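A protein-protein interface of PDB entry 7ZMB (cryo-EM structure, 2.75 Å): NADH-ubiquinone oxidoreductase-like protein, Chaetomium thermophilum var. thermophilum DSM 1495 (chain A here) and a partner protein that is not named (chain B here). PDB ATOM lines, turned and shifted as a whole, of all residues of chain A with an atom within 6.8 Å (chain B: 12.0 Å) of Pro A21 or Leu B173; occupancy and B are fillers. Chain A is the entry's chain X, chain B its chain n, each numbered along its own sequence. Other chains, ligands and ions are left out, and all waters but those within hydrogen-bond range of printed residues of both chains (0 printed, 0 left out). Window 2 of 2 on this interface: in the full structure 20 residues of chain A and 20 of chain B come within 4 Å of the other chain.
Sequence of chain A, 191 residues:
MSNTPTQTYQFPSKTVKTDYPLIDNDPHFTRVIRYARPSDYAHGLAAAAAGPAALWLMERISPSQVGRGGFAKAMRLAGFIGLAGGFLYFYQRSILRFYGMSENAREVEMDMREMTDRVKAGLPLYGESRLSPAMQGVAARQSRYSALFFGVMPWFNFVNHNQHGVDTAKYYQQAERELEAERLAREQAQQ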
ATOM      1  N   THR A  18      18.997 -19.863  14.796  1.00  0.00           N
ATOM      2  CA  THR A  18      19.751 -19.425  13.590  1.00  0.00           C
ATOM      3  C   THR A  18      20.957 -18.591  14.035  1.00  0.00           C
ATOM      4  O   THR A  18      20.932 -18.113  15.173  1.00  0.00           O
ATOM      5  CB  THR A  18      18.835 -18.690  12.600  1.00  0.00           C
ATOM      6  OG1 THR A  18      18.474 -17.422  13.146  1.00  0.00           O
ATOM      7  CG2 THR A  18      17.587 -19.464  12.241  1.00  0.00           C
ATOM      8  N   ASP A  19      21.969 -18.447  13.174  1.00  0.00           N
ATOM      9  CA  ASP A  19      23.172 -17.644  13.510  1.00  0.00           C
ATOM     10  C   ASP A  19      22.884 -16.140  13.532  1.00  0.00           C
ATOM     11  O   ASP A  19      23.351 -15.469  14.465  1.00  0.00           O
ATOM     12  CB  ASP A  19      24.334 -17.974  12.577  1.00  0.00           C
ATOM     13  CG  ASP A  19      24.637 -19.460  12.498  1.00  0.00           C
ATOM     14  OD1 ASP A  19      24.257 -20.185  13.439  1.00  0.00           O
ATOM     15  OD2 ASP A  19      25.239 -19.882  11.492  1.00  0.00           O
ATOM     16  N   TYR A  20      22.127 -15.628  12.564  1.00  0.00           N
ATOM     17  CA  TYR A  20      21.953 -14.152  12.486  1.00  0.00           C
ATOM     18  C   TYR A  20      20.594 -13.698  13.023  1.00  0.00           C
ATOM     19  O   TYR A  20      19.715 -14.543  13.234  1.00  0.00           O
ATOM     20  CB  TYR A  20      22.262 -13.679  11.068  1.00  0.00           C
ATOM     21  CG  TYR A  20      23.609 -14.120  10.557  1.00  0.00           C
ATOM     22  CD1 TYR A  20      24.711 -13.284  10.629  1.00  0.00           C
ATOM     23  CD2 TYR A  20      23.786 -15.379  10.009  1.00  0.00           C
ATOM     24  CE1 TYR A  20      25.951 -13.686  10.164  1.00  0.00           C
ATOM     25  CE2 TYR A  20      25.019 -15.796   9.538  1.00  0.00           C
ATOM     26  CZ  TYR A  20      26.106 -14.947   9.616  1.00  0.00           C
ATOM     27  OH  TYR A  20      27.326 -15.349   9.156  1.00  0.00           O
ATOM     28  N   PRO A  21      20.461 -12.391  13.330  1.00  0.00           N
ATOM     29  CA  PRO A  21      19.188 -11.814  13.757  1.00  0.00           C
ATOM     30  C   PRO A  21      17.995 -11.979  12.811  1.00  0.00           C
ATOM     31  O   PRO A  21      18.165 -11.860  11.621  1.00  0.00           O
ATOM     32  CB  PRO A  21      19.516 -10.316  13.875  1.00  0.00           C
ATOM     33  CG  PRO A  21      20.811 -10.118  13.132  1.00  0.00           C
ATOM     34  CD  PRO A  21      21.551 -11.420  13.311  1.00  0.00           C
ATOM     35  N   LEU A  22      16.821 -12.239  13.387  1.00  0.00           N
ATOM     36  CA  LEU A  22      15.596 -12.410  12.572  1.00  0.00           C
ATOM     37  C   LEU A  22      14.993 -11.036  12.284  1.00  0.00           C
ATOM     38  O   LEU A  22      14.773 -10.280  13.236  1.00  0.00           O
ATOM     39  CB  LEU A  22      14.603 -13.317  13.305  1.00  0.00           C
ATOM     40  CG  LEU A  22      13.201 -13.382  12.693  1.00  0.00           C
ATOM     41  CD1 LEU A  22      13.208 -14.130  11.369  1.00  0.00           C
ATOM     42  CD2 LEU A  22      12.203 -14.006  13.654  1.00  0.00           C
ATOM     43  N   ILE A  23      14.771 -10.734  11.005  1.00  0.00           N
ATOM     44  CA  ILE A  23      14.147  -9.440  10.604  1.00  0.00           C
ATOM     45  C   ILE A  23      12.677  -9.698  10.286  1.00  0.00           C
ATOM     46  O   ILE A  23      11.829  -8.973  10.807  1.00  0.00           O
ATOM     47  CB  ILE A  23      14.874  -8.904   9.359  1.00  0.00           C
ATOM     48  CG1 ILE A  23      16.334  -8.545   9.635  1.00  0.00           C
ATOM     49  CG2 ILE A  23      14.111  -7.765   8.720  1.00  0.00           C
ATOM     50  CD1 ILE A  23      17.163  -8.454   8.382  1.00  0.00           C
ATOM     51  N   ASP A  24      12.402 -10.722   9.487  1.00  0.00           N
ATOM     52  CA  ASP A  24      11.022 -10.980   9.021  1.00  0.00           C
ATOM     53  C   ASP A  24      10.925 -12.443   8.595  1.00  0.00           C
ATOM     54  O   ASP A  24      11.645 -12.817   7.661  1.00  0.00           O
ATOM     55  CB  ASP A  24      10.668 -10.001   7.909  1.00  0.00           C
ATOM     56  CG  ASP A  24       9.198  -9.942   7.577  1.00  0.00           C
ATOM     57  OD1 ASP A  24       8.547 -10.981   7.683  1.00  0.00           O
ATOM     58  OD2 ASP A  24       8.728  -8.853   7.223  1.00  0.00           O
ATOM     59  N   LEU A  96      16.812 -15.511   2.982  1.00  0.00           N
ATOM     60  CA  LEU A  96      17.573 -16.105   4.117  1.00  0.00           C
ATOM     61  C   LEU A  96      18.165 -14.986   4.987  1.00  0.00           C
ATOM     62  O   LEU A  96      18.229 -15.187   6.208  1.00  0.00           O
ATOM     63  CB  LEU A  96      18.606 -17.118   3.625  1.00  0.00           C
ATOM     64  CG  LEU A  96      18.267 -18.590   3.850  1.00  0.00           C
ATOM     65  CD1 LEU A  96      16.947 -18.954   3.191  1.00  0.00           C
ATOM     66  CD2 LEU A  96      19.381 -19.476   3.322  1.00  0.00           C
ATOM     67  N   ARG A  97      18.592 -13.869   4.388  1.00  0.00           N
ATOM     68  CA  ARG A  97      19.099 -12.696   5.156  1.00  0.00           C
ATOM     69  C   ARG A  97      17.948 -12.098   5.972  1.00  0.00           C
ATOM     70  O   ARG A  97      18.219 -11.444   6.986  1.00  0.00           O
ATOM     71  CB  ARG A  97      19.817 -11.704   4.236  1.00  0.00           C
ATOM     72  CG  ARG A  97      20.897 -12.339   3.375  1.00  0.00           C
ATOM     73  CD  ARG A  97      21.788 -11.345   2.662  1.00  0.00           C
ATOM     74  NE  ARG A  97      22.578 -12.010   1.640  1.00  0.00           N
ATOM     75  CZ  ARG A  97      22.266 -12.042   0.350  1.00  0.00           C
ATOM     76  NH1 ARG A  97      21.180 -11.428  -0.085  1.00  0.00           N
ATOM     77  NH2 ARG A  97      23.044 -12.683  -0.501  1.00  0.00           N
ATOM     78  N   PHE A  98      16.713 -12.357   5.560  1.00  0.00           N
ATOM     79  CA  PHE A  98      15.508 -11.872   6.280  1.00  0.00           C
ATOM     80  C   PHE A  98      15.160 -12.923   7.332  1.00  0.00           C
ATOM     81  O   PHE A  98      14.660 -12.540   8.401  1.00  0.00           O
ATOM     82  CB  PHE A  98      14.354 -11.658   5.297  1.00  0.00           C
ATOM     83  CG  PHE A  98      14.224 -10.287   4.688  1.00  0.00           C
ATOM     84  CD1 PHE A  98      13.871  -9.195   5.463  1.00  0.00           C
ATOM     85  CD2 PHE A  98      14.402 -10.098   3.327  1.00  0.00           C
ATOM     86  CE1 PHE A  98      13.735  -7.938   4.896  1.00  0.00           C
ATOM     87  CE2 PHE A  98      14.261  -8.841   2.761  1.00  0.00           C
ATOM     88  CZ  PHE A  98      13.928  -7.764   3.546  1.00  0.00           C
ATOM     89  N   TYR A  99      15.424 -14.200   7.033  1.00  0.00           N
ATOM     90  CA  TYR A  99      15.162 -15.303   7.948  1.00  0.00           C
ATOM     91  C   TYR A  99      16.176 -15.394   9.077  1.00  0.00           C
ATOM     92  O   TYR A  99      15.991 -16.211   9.983  1.00  0.00           O
ATOM     93  CB  TYR A  99      15.170 -16.632   7.195  1.00  0.00           C
ATOM     94  CG  TYR A  99      13.958 -16.921   6.346  1.00  0.00           C
ATOM     95  CD1 TYR A  99      12.839 -16.108   6.390  1.00  0.00           C
ATOM     96  CD2 TYR A  99      13.933 -18.027   5.508  1.00  0.00           C
ATOM     97  CE1 TYR A  99      11.746 -16.373   5.619  1.00  0.00           C
ATOM     98  CE2 TYR A  99      12.831 -18.305   4.733  1.00  0.00           C
ATOM     99  CZ  TYR A  99      11.740 -17.476   4.793  1.00  0.00           C
ATOM    100  OH  TYR A  99      10.638 -17.744   4.024  1.00  0.00           O
ATOM    101  N   GLY A 100      17.249 -14.609   9.032  1.00  0.00           N
ATOM    102  CA  GLY A 100      18.301 -14.753  10.009  1.00  0.00           C
ATOM    103  C   GLY A 100      19.152 -15.976   9.815  1.00  0.00           C
ATOM    104  O   GLY A 100      19.832 -16.399  10.747  1.00  0.00           O
ATOM    105  N   MET A 101      19.095 -16.550   8.614  1.00  0.00           N
ATOM    106  CA  MET A 101      19.836 -17.791   8.301  1.00  0.00           C
ATOM    107  C   MET A 101      20.984 -17.491   7.342  1.00  0.00           C
ATOM    108  O   MET A 101      21.467 -18.427   6.698  1.00  0.00           O
ATOM    109  CB  MET A 101      18.857 -18.792   7.688  1.00  0.00           C
ATOM    110  CG  MET A 101      17.632 -19.012   8.541  1.00  0.00           C
ATOM    111  SD  MET A 101      16.619 -20.365   7.921  1.00  0.00           S
ATOM    112  CE  MET A 101      15.254 -20.300   9.080  1.00  0.00           C
ATOM    113  N   SER A 102      21.362 -16.228   7.209  1.00  0.00           N
ATOM    114  CA  SER A 102      22.539 -15.828   6.398  1.00  0.00           C
ATOM    115  C   SER A 102      23.066 -14.521   7.014  1.00  0.00           C
ATOM    116  O   SER A 102      22.291 -13.883   7.738  1.00  0.00           O
ATOM    117  CB  SER A 102      22.162 -15.692   4.941  1.00  0.00           C
ATOM    118  OG  SER A 102      23.222 -15.124   4.184  1.00  0.00           O
ATOM    119  N   ASN A 104      23.493 -10.905   7.582  1.00  0.00           N
ATOM    120  CA  ASN A 104      22.519  -9.927   7.114  1.00  0.00           C
ATOM    121  C   ASN A 104      22.720  -8.548   7.727  1.00  0.00           C
ATOM    122  O   ASN A 104      21.746  -7.836   7.974  1.00  0.00           O
ATOM    123  CB  ASN A 104      21.100 -10.423   7.387  1.00  0.00           C
ATOM    124  CG  ASN A 104      20.806 -10.589   8.867  1.00  0.00           C
ATOM    125  OD1 ASN A 104      21.680 -10.416   9.709  1.00  0.00           O
ATOM    126  ND2 ASN A 104      19.568 -10.926   9.188  1.00  0.00           N
ATOM    127  N   ALA A 105      23.968  -8.142   7.966  1.00  0.00           N
ATOM    128  CA  ALA A 105      24.201  -6.867   8.640  1.00  0.00           C
ATOM    129  C   ALA A 105      23.623  -5.710   7.844  1.00  0.00           C
ATOM    130  O   ALA A 105      22.997  -4.806   8.409  1.00  0.00           O
ATOM    131  CB  ALA A 105      25.694  -6.660   8.873  1.00  0.00           C
ATOM    132  N   VAL A 108      19.695  -5.673   8.145  1.00  0.00           N
ATOM    133  CA  VAL A 108      19.159  -5.247   9.435  1.00  0.00           C
ATOM    134  C   VAL A 108      19.074  -3.728   9.510  1.00  0.00           C
ATOM    135  O   VAL A 108      18.073  -3.172   9.972  1.00  0.00           O
ATOM    136  CB  VAL A 108      20.004  -5.822  10.586  1.00  0.00           C
ATOM    137  CG1 VAL A 108      19.466  -5.354  11.924  1.00  0.00           C
ATOM    138  CG2 VAL A 108      19.992  -7.316  10.541  1.00  0.00           C
ATOM    139  N   LYS A 170      11.032  -2.377  19.034  1.00  0.00           N
ATOM    140  CA  LYS A 170      12.330  -1.748  18.718  1.00  0.00           C
ATOM    141  C   LYS A 170      12.136  -0.639  17.679  1.00  0.00           C
ATOM    142  O   LYS A 170      12.795   0.390  17.825  1.00  0.00           O
ATOM    143  CB  LYS A 170      13.304  -2.807  18.194  1.00  0.00           C
ATOM    144  CG  LYS A 170      12.794  -3.627  17.017  1.00  0.00           C
ATOM    145  CD  LYS A 170      13.785  -4.638  16.511  1.00  0.00           C
ATOM    146  CE  LYS A 170      13.201  -5.531  15.440  1.00  0.00           C
ATOM    147  NZ  LYS A 170      14.086  -6.682  15.153  1.00  0.00           N
ATOM    148  N   GLN B 161      10.285 -16.505  24.305  1.00  0.00           N
ATOM    149  CA  GLN B 161      11.192 -17.361  23.502  1.00  0.00           C
ATOM    150  C   GLN B 161      11.822 -16.512  22.393  1.00  0.00           C
ATOM    151  O   GLN B 161      13.051 -16.600  22.237  1.00  0.00           O
ATOM    152  CB  GLN B 161      10.453 -18.606  23.007  1.00  0.00           C
ATOM    153  CG  GLN B 161      11.349 -19.667  22.394  1.00  0.00           C
ATOM    154  CD  GLN B 161      10.542 -20.800  21.808  1.00  0.00           C
ATOM    155  OE1 GLN B 161      11.077 -21.715  21.188  1.00  0.00           O
ATOM    156  NE2 GLN B 161       9.235 -20.743  22.001  1.00  0.00           N
ATOM    157  N   HIS B 162      11.026 -15.733  21.653  1.00  0.00           N
ATOM    158  CA  HIS B 162      11.600 -14.841  20.611  1.00  0.00           C
ATOM    159  C   HIS B 162      12.594 -13.842  21.214  1.00  0.00           C
ATOM    160  O   HIS B 162      13.725 -13.805  20.723  1.00  0.00           O
ATOM    161  CB  HIS B 162      10.490 -14.116  19.832  1.00  0.00           C
ATOM    162  CG  HIS B 162      10.977 -13.066  18.893  1.00  0.00           C
ATOM    163  ND1 HIS B 162      11.666 -13.367  17.740  1.00  0.00           N
ATOM    164  CD2 HIS B 162      10.854 -11.725  18.921  1.00  0.00           C
ATOM    165  CE1 HIS B 162      11.962 -12.252  17.105  1.00  0.00           C
ATOM    166  NE2 HIS B 162      11.479 -11.231  17.811  1.00  0.00           N
ATOM    167  N   LEU B 163      12.245 -13.162  22.301  1.00  0.00           N
ATOM    168  CA  LEU B 163      13.160 -12.186  22.945  1.00  0.00           C
ATOM    169  C   LEU B 163      14.442 -12.891  23.394  1.00  0.00           C
ATOM    170  O   LEU B 163      15.516 -12.333  23.148  1.00  0.00           O
ATOM    171  CB  LEU B 163      12.462 -11.576  24.161  1.00  0.00           C
ATOM    172  CG  LEU B 163      11.892 -10.170  24.000  1.00  0.00           C
ATOM    173  CD1 LEU B 163      12.941  -9.217  23.453  1.00  0.00           C
ATOM    174  CD2 LEU B 163      10.644 -10.171  23.135  1.00  0.00           C
ATOM    175  N   GLU B 164      14.323 -14.072  23.997  1.00  0.00           N
ATOM    176  CA  GLU B 164      15.478 -14.810  24.558  1.00  0.00           C
ATOM    177  C   GLU B 164      16.458 -15.215  23.462  1.00  0.00           C
ATOM    178  O   GLU B 164      17.660 -15.049  23.673  1.00  0.00           O
ATOM    179  CB  GLU B 164      14.984 -16.059  25.288  1.00  0.00           C
ATOM    180  CG  GLU B 164      14.495 -15.783  26.697  1.00  0.00           C
ATOM    181  CD  GLU B 164      15.575 -15.380  27.688  1.00  0.00           C
ATOM    182  OE1 GLU B 164      15.237 -14.716  28.688  1.00  0.00           O
ATOM    183  OE2 GLU B 164      16.748 -15.741  27.464  1.00  0.00           O
ATOM    184  N   GLU B 165      15.950 -15.759  22.361  1.00  0.00           N
ATOM    185  CA  GLU B 165      16.751 -16.270  21.219  1.00  0.00           C
ATOM    186  C   GLU B 165      17.457 -15.085  20.565  1.00  0.00           C
ATOM    187  O   GLU B 165      18.641 -15.221  20.234  1.00  0.00           O
ATOM    188  CB  GLU B 165      15.824 -16.985  20.229  1.00  0.00           C
ATOM    189  CG  GLU B 165      16.420 -17.206  18.853  1.00  0.00           C
ATOM    190  CD  GLU B 165      17.297 -18.434  18.703  1.00  0.00           C
ATOM    191  OE1 GLU B 165      17.179 -19.352  19.539  1.00  0.00           O
ATOM    192  OE2 GLU B 165      18.091 -18.473  17.744  1.00  0.00           O
ATOM    193  N   GLU B 166      16.755 -13.960  20.419  1.00  0.00           N
ATOM    194  CA  GLU B 166      17.306 -12.749  19.756  1.00  0.00           C
ATOM    195  C   GLU B 166      18.336 -12.128  20.692  1.00  0.00           C
ATOM    196  O   GLU B 166      19.363 -11.654  20.207  1.00  0.00           O
ATOM    197  CB  GLU B 166      16.185 -11.755  19.439  1.00  0.00           C
ATOM    198  CG  GLU B 166      15.154 -12.272  18.455  1.00  0.00           C
ATOM    199  CD  GLU B 166      15.667 -12.820  17.135  1.00  0.00           C
ATOM    200  OE1 GLU B 166      16.662 -12.287  16.611  1.00  0.00           O
ATOM    201  OE2 GLU B 166      15.063 -13.788  16.634  1.00  0.00           O
ATOM    202  N   GLU B 167      18.038 -12.132  21.985  1.00  0.00           N
ATOM    203  CA  GLU B 167      18.989 -11.627  23.002  1.00  0.00           C
ATOM    204  C   GLU B 167      20.208 -12.534  22.956  1.00  0.00           C
ATOM    205  O   GLU B 167      21.329 -12.013  22.874  1.00  0.00           O
ATOM    206  CB  GLU B 167      18.393 -11.779  24.398  1.00  0.00           C
ATOM    207  CG  GLU B 167      19.262 -11.197  25.496  1.00  0.00           C
ATOM    208  CD  GLU B 167      18.776 -11.485  26.906  1.00  0.00           C
ATOM    209  OE1 GLU B 167      17.736 -12.159  27.045  1.00  0.00           O
ATOM    210  OE2 GLU B 167      19.441 -11.036  27.861  1.00  0.00           O
ATOM    211  N   ARG B 168      19.989 -13.844  22.983  1.00  0.00           N
ATOM    212  CA  ARG B 168      21.123 -14.793  22.871  1.00  0.00           C
ATOM    213  C   ARG B 168      21.935 -14.459  21.619  1.00  0.00           C
ATOM    214  O   ARG B 168      23.177 -14.476  21.703  1.00  0.00           O
ATOM    215  CB  ARG B 168      20.598 -16.229  22.816  1.00  0.00           C
ATOM    216  CG  ARG B 168      21.683 -17.293  22.763  1.00  0.00           C
ATOM    217  CD  ARG B 168      21.130 -18.608  22.249  1.00  0.00           C
ATOM    218  NE  ARG B 168      20.601 -18.485  20.898  1.00  0.00           N
ATOM    219  CZ  ARG B 168      21.329 -18.611  19.795  1.00  0.00           C
ATOM    220  NH1 ARG B 168      20.761 -18.489  18.608  1.00  0.00           N
ATOM    221  NH2 ARG B 168      22.624 -18.862  19.880  1.00  0.00           N
ATOM    222  N   LYS B 169      21.265 -14.147  20.509  1.00  0.00           N
ATOM    223  CA  LYS B 169      21.980 -13.938  19.260  1.00  0.00           C
ATOM    224  C   LYS B 169      22.771 -12.643  19.286  1.00  0.00           C
ATOM    225  O   LYS B 169      23.870 -12.575  18.727  1.00  0.00           O
ATOM    226  CB  LYS B 169      21.001 -13.956  18.093  1.00  0.00           C
ATOM    227  CG  LYS B 169      20.721 -15.351  17.579  1.00  0.00           C
ATOM    228  CD  LYS B 169      19.955 -15.308  16.291  1.00  0.00           C
ATOM    229  CE  LYS B 169      18.469 -15.369  16.548  1.00  0.00           C
ATOM    230  NZ  LYS B 169      17.686 -15.209  15.301  1.00  0.00           N
ATOM    231  N   ALA B 170      22.233 -11.614  19.941  1.00  0.00           N
ATOM    232  CA  ALA B 170      22.919 -10.336  20.004  1.00  0.00           C
ATOM    233  C   ALA B 170      24.121 -10.373  20.933  1.00  0.00           C
ATOM    234  O   ALA B 170      25.035  -9.558  20.776  1.00  0.00           O
ATOM    235  CB  ALA B 170      21.947  -9.243  20.447  1.00  0.00           C
ATOM    236  N   LYS B 171      24.146 -11.295  21.888  1.00  0.00           N
ATOM    237  CA  LYS B 171      25.280 -11.443  22.787  1.00  0.00           C
ATOM    238  C   LYS B 171      26.360 -12.359  22.229  1.00  0.00           C
ATOM    239  O   LYS B 171      27.369 -12.582  22.904  1.00  0.00           O
ATOM    240  CB  LYS B 171      24.814 -11.964  24.150  1.00  0.00           C
ATOM    241  CG  LYS B 171      24.198 -10.897  25.039  1.00  0.00           C
ATOM    242  CD  LYS B 171      23.975 -11.407  26.454  1.00  0.00           C
ATOM    243  CE  LYS B 171      22.772 -12.331  26.523  1.00  0.00           C
ATOM    244  NZ  LYS B 171      22.395 -12.651  27.927  1.00  0.00           N
ATOM    245  N   LYS B 172      26.174 -12.896  21.026  1.00  0.00           N
ATOM    246  CA  LYS B 172      27.190 -13.716  20.383  1.00  0.00           C
ATOM    247  C   LYS B 172      27.931 -12.998  19.270  1.00  0.00           C
ATOM    248  O   LYS B 172      29.151 -13.139  19.170  1.00  0.00           O
ATOM    249  CB  LYS B 172      26.566 -14.997  19.816  1.00  0.00           C
ATOM    250  CG  LYS B 172      27.573 -15.972  19.248  1.00  0.00           C
ATOM    251  CD  LYS B 172      26.896 -17.242  18.758  1.00  0.00           C
ATOM    252  CE  LYS B 172      27.912 -18.233  18.221  1.00  0.00           C
ATOM    253  NZ  LYS B 172      28.568 -17.728  16.985  1.00  0.00           N
ATOM    254  N   LEU B 173      27.234 -12.230  18.439  1.00  0.00           N
ATOM    255  CA  LEU B 173      27.878 -11.461  17.386  1.00  0.00           C
ATOM    256  C   LEU B 173      28.603 -10.234  17.920  1.00  0.00           C
ATOM    257  O   LEU B 173      29.376  -9.618  17.180  1.00  0.00           O
ATOM    258  CB  LEU B 173      26.852 -11.051  16.322  1.00  0.00           C
ATOM    259  CG  LEU B 173      25.611 -10.252  16.727  1.00  0.00           C
ATOM    260  CD1 LEU B 173      25.885  -8.754  16.747  1.00  0.00           C
ATOM    261  CD2 LEU B 173      24.462 -10.569  15.784  1.00  0.00           C
ATOM    262  N   ALA B 174      28.373  -9.864  19.178  1.00  0.00           N
ATOM    263  CA  ALA B 174      29.154  -8.822  19.828  1.00  0.00           C
ATOM    264  C   ALA B 174      30.428  -9.353  20.462  1.00  0.00           C
ATOM    265  O   ALA B 174      31.412  -8.614  20.563  1.00  0.00           O
ATOM    266  CB  ALA B 174      28.316  -8.112  20.897  1.00  0.00           C
ATOM    267  N   ALA B 175      30.431 -10.617  20.894  1.00  0.00           N
ATOM    268  CA  ALA B 175      31.662 -11.228  21.384  1.00  0.00           C
ATOM    269  C   ALA B 175      32.689 -11.355  20.267  1.00  0.00           C
ATOM    270  O   ALA B 175      33.893 -11.184  20.496  1.00  0.00           O
ATOM    271  CB  ALA B 175      31.366 -12.593  22.002  1.00  0.00           C
ATOM    272  N   ALA B 176      32.233 -11.664  19.050  1.00  0.00           N
ATOM    273  CA  ALA B 176      33.141 -11.706  17.909  1.00  0.00           C
ATOM    274  C   ALA B 176      33.745 -10.334  17.640  1.00  0.00           C
ATOM    275  O   ALA B 176      34.918 -10.226  17.264  1.00  0.00           O
ATOM    276  CB  ALA B 176      32.411 -12.225  16.671  1.00  0.00           C
ATOM    277  N   ALA B 177      32.955  -9.273  17.819  1.00  0.00           N
ATOM    278  CA  ALA B 177      33.496  -7.923  17.702  1.00  0.00           C
ATOM    279  C   ALA B 177      34.561  -7.667  18.761  1.00  0.00           C
ATOM    280  O   ALA B 177      35.589  -7.041  18.481  1.00  0.00           O
ATOM    281  CB  ALA B 177      32.372  -6.893  17.806  1.00  0.00           C
ATOM    282  N   ALA B 178      34.326  -8.136  19.989  1.00  0.00           N
ATOM    283  CA  ALA B 178      35.349  -8.035  21.023  1.00  0.00           C
ATOM    284  C   ALA B 178      36.573  -8.870  20.666  1.00  0.00           C
ATOM    285  O   ALA B 178      37.712  -8.437  20.877  1.00  0.00           O
ATOM    286  CB  ALA B 178      34.777  -8.466  22.373  1.00  0.00           C
ATOM    287  N   ALA B 179      36.358 -10.068  20.125  1.00  0.00           N
ATOM    288  CA  ALA B 179      37.455 -10.950  19.724  1.00  0.00           C
ATOM    289  C   ALA B 179      37.840 -10.661  18.273  1.00  0.00           C
ATOM    290  O   ALA B 179      37.738 -11.502  17.379  1.00  0.00           O
ATOM    291  CB  ALA B 179      37.066 -12.408  19.926  1.00  0.00           C
ATOM    292  N   ALA B 180      38.295  -9.432  18.055  1.00  0.00           N
ATOM    293  CA  ALA B 180      38.705  -8.994  16.725  1.00  0.00           C
ATOM    294  C   ALA B 180      40.126  -8.442  16.747  1.00  0.00           C
ATOM    295  O   ALA B 180      40.644  -7.995  15.724  1.00  0.00           O
ATOM    296  CB  ALA B 180      37.739  -7.950  16.189  1.00  0.00           C
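Pro A21 touches just these residues of chain B: Glu B166 (3.8 Å) and Leu B173 (3.9 Å). Of the printed residues of chain B, Thr A18 touches Glu B165 (3.4 Å), Arg B168 (3.5 Å) and Lys B169 (3.2 Å). Leu A22 touches just these residues of chain B: His B162, Glu B166 and Lys B169. No residue of chain B comes within 4 Å of Gly A100. No residue of chain B comes within 4 Å of Asn A104. No residue of chain B comes within 4 Å of Ala A105. Printed residues of chain A within 4 Å of Glu B165: Thr A18. Of the printed residues of chain A, Arg B168 touches Thr A18. Of the printed residues of chain A, Lys B169 touches Thr A18 (3.2 Å), Asp A19 (3.9 Å), Tyr A20 (3.0 Å) and Leu A22 (3.6 Å). Of the printed residues of chain A, His B162 touches Leu A22. Of the printed residues of chain A, Glu B166 touches Pro A21 (3.8 Å) and Leu A22 (3.2 Å). Glu B167 touches none of the printed residues of chain A. Lys B171 touches none of the printed residues of chain A. The nearest residue of chain A that does not touch Leu B173 is Asp A19 (5.2 Å).
The backbone carbonyl oxygen (O) of Tyr A20 lies within hydrogen-bond range of the side-chain hydroxyl (OG1) of Thr A18 (3.1 Å). The side-chain hydroxyl (OG1) of Thr A18 lies within hydrogen-bond range of the backbone carbonyl oxygen (O) of Gly A100. The backbone NH (N) of Tyr A20 sits at hydrogen-bond distance from the backbone carbonyl oxygen (O) of Gly A100, at 3.0 Å. The side-chain amide nitrogen of Asn A104 sits at hydrogen-bond distance from the backbone carbonyl oxygen of Pro A21, at 3.0 Å. The guanidinium group of Arg B168 lies within salt-bridge range of the side-chain carboxylate of Glu B165 (2.8 Å). The side-chain carboxylate (OE2) of Glu B166 lies within salt-bridge range of the side-chain amino group (NZ) of Lys B169, at 3.3 Å.
Printed residues of chain B that touch a printed residue of chain A: His B162, Glu B165, Glu B166, Arg B168, Lys B169 and Leu B173. Hydrophobic or aromatic side chains of chain B within 4 Å of the printed part of chain A: His B162 and Leu B173. Of the 18 printed residues of chain A, 5 touch a printed residue of chain B. Among the printed residues, 10 pairs touch across the chains.
The backbone NH (N) of Thr A18 lies within hydrogen-bond range of the side-chain carboxylate (OE2) of Glu B165, at 3.4 Å. The guanidinium group (NH1) of Arg B168 sits at hydrogen-bond distance from the backbone carbonyl oxygen (O) of Thr A18 (3.5 Å). NZ of Lys B169 sits at hydrogen-bond distance from OG1 of Thr A18. O of Tyr A20 sits at hydrogen-bond distance from NZ of Lys B169, 3.0 Å away. OE1 of Glu B166 is in hydrogen-bond range of N of Leu A22, at 3.2 Å.
CD of Lys B169 touches O of Asp A19 (3.9 Å). OE1 of Glu B166 touches CA of Pro A21, 3.8 Å away. Leu B173 touches Pro A21. CE1 of His B162 touches CD2 of Leu A22 (3.9 Å). Leu A22 touches Lys B169.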
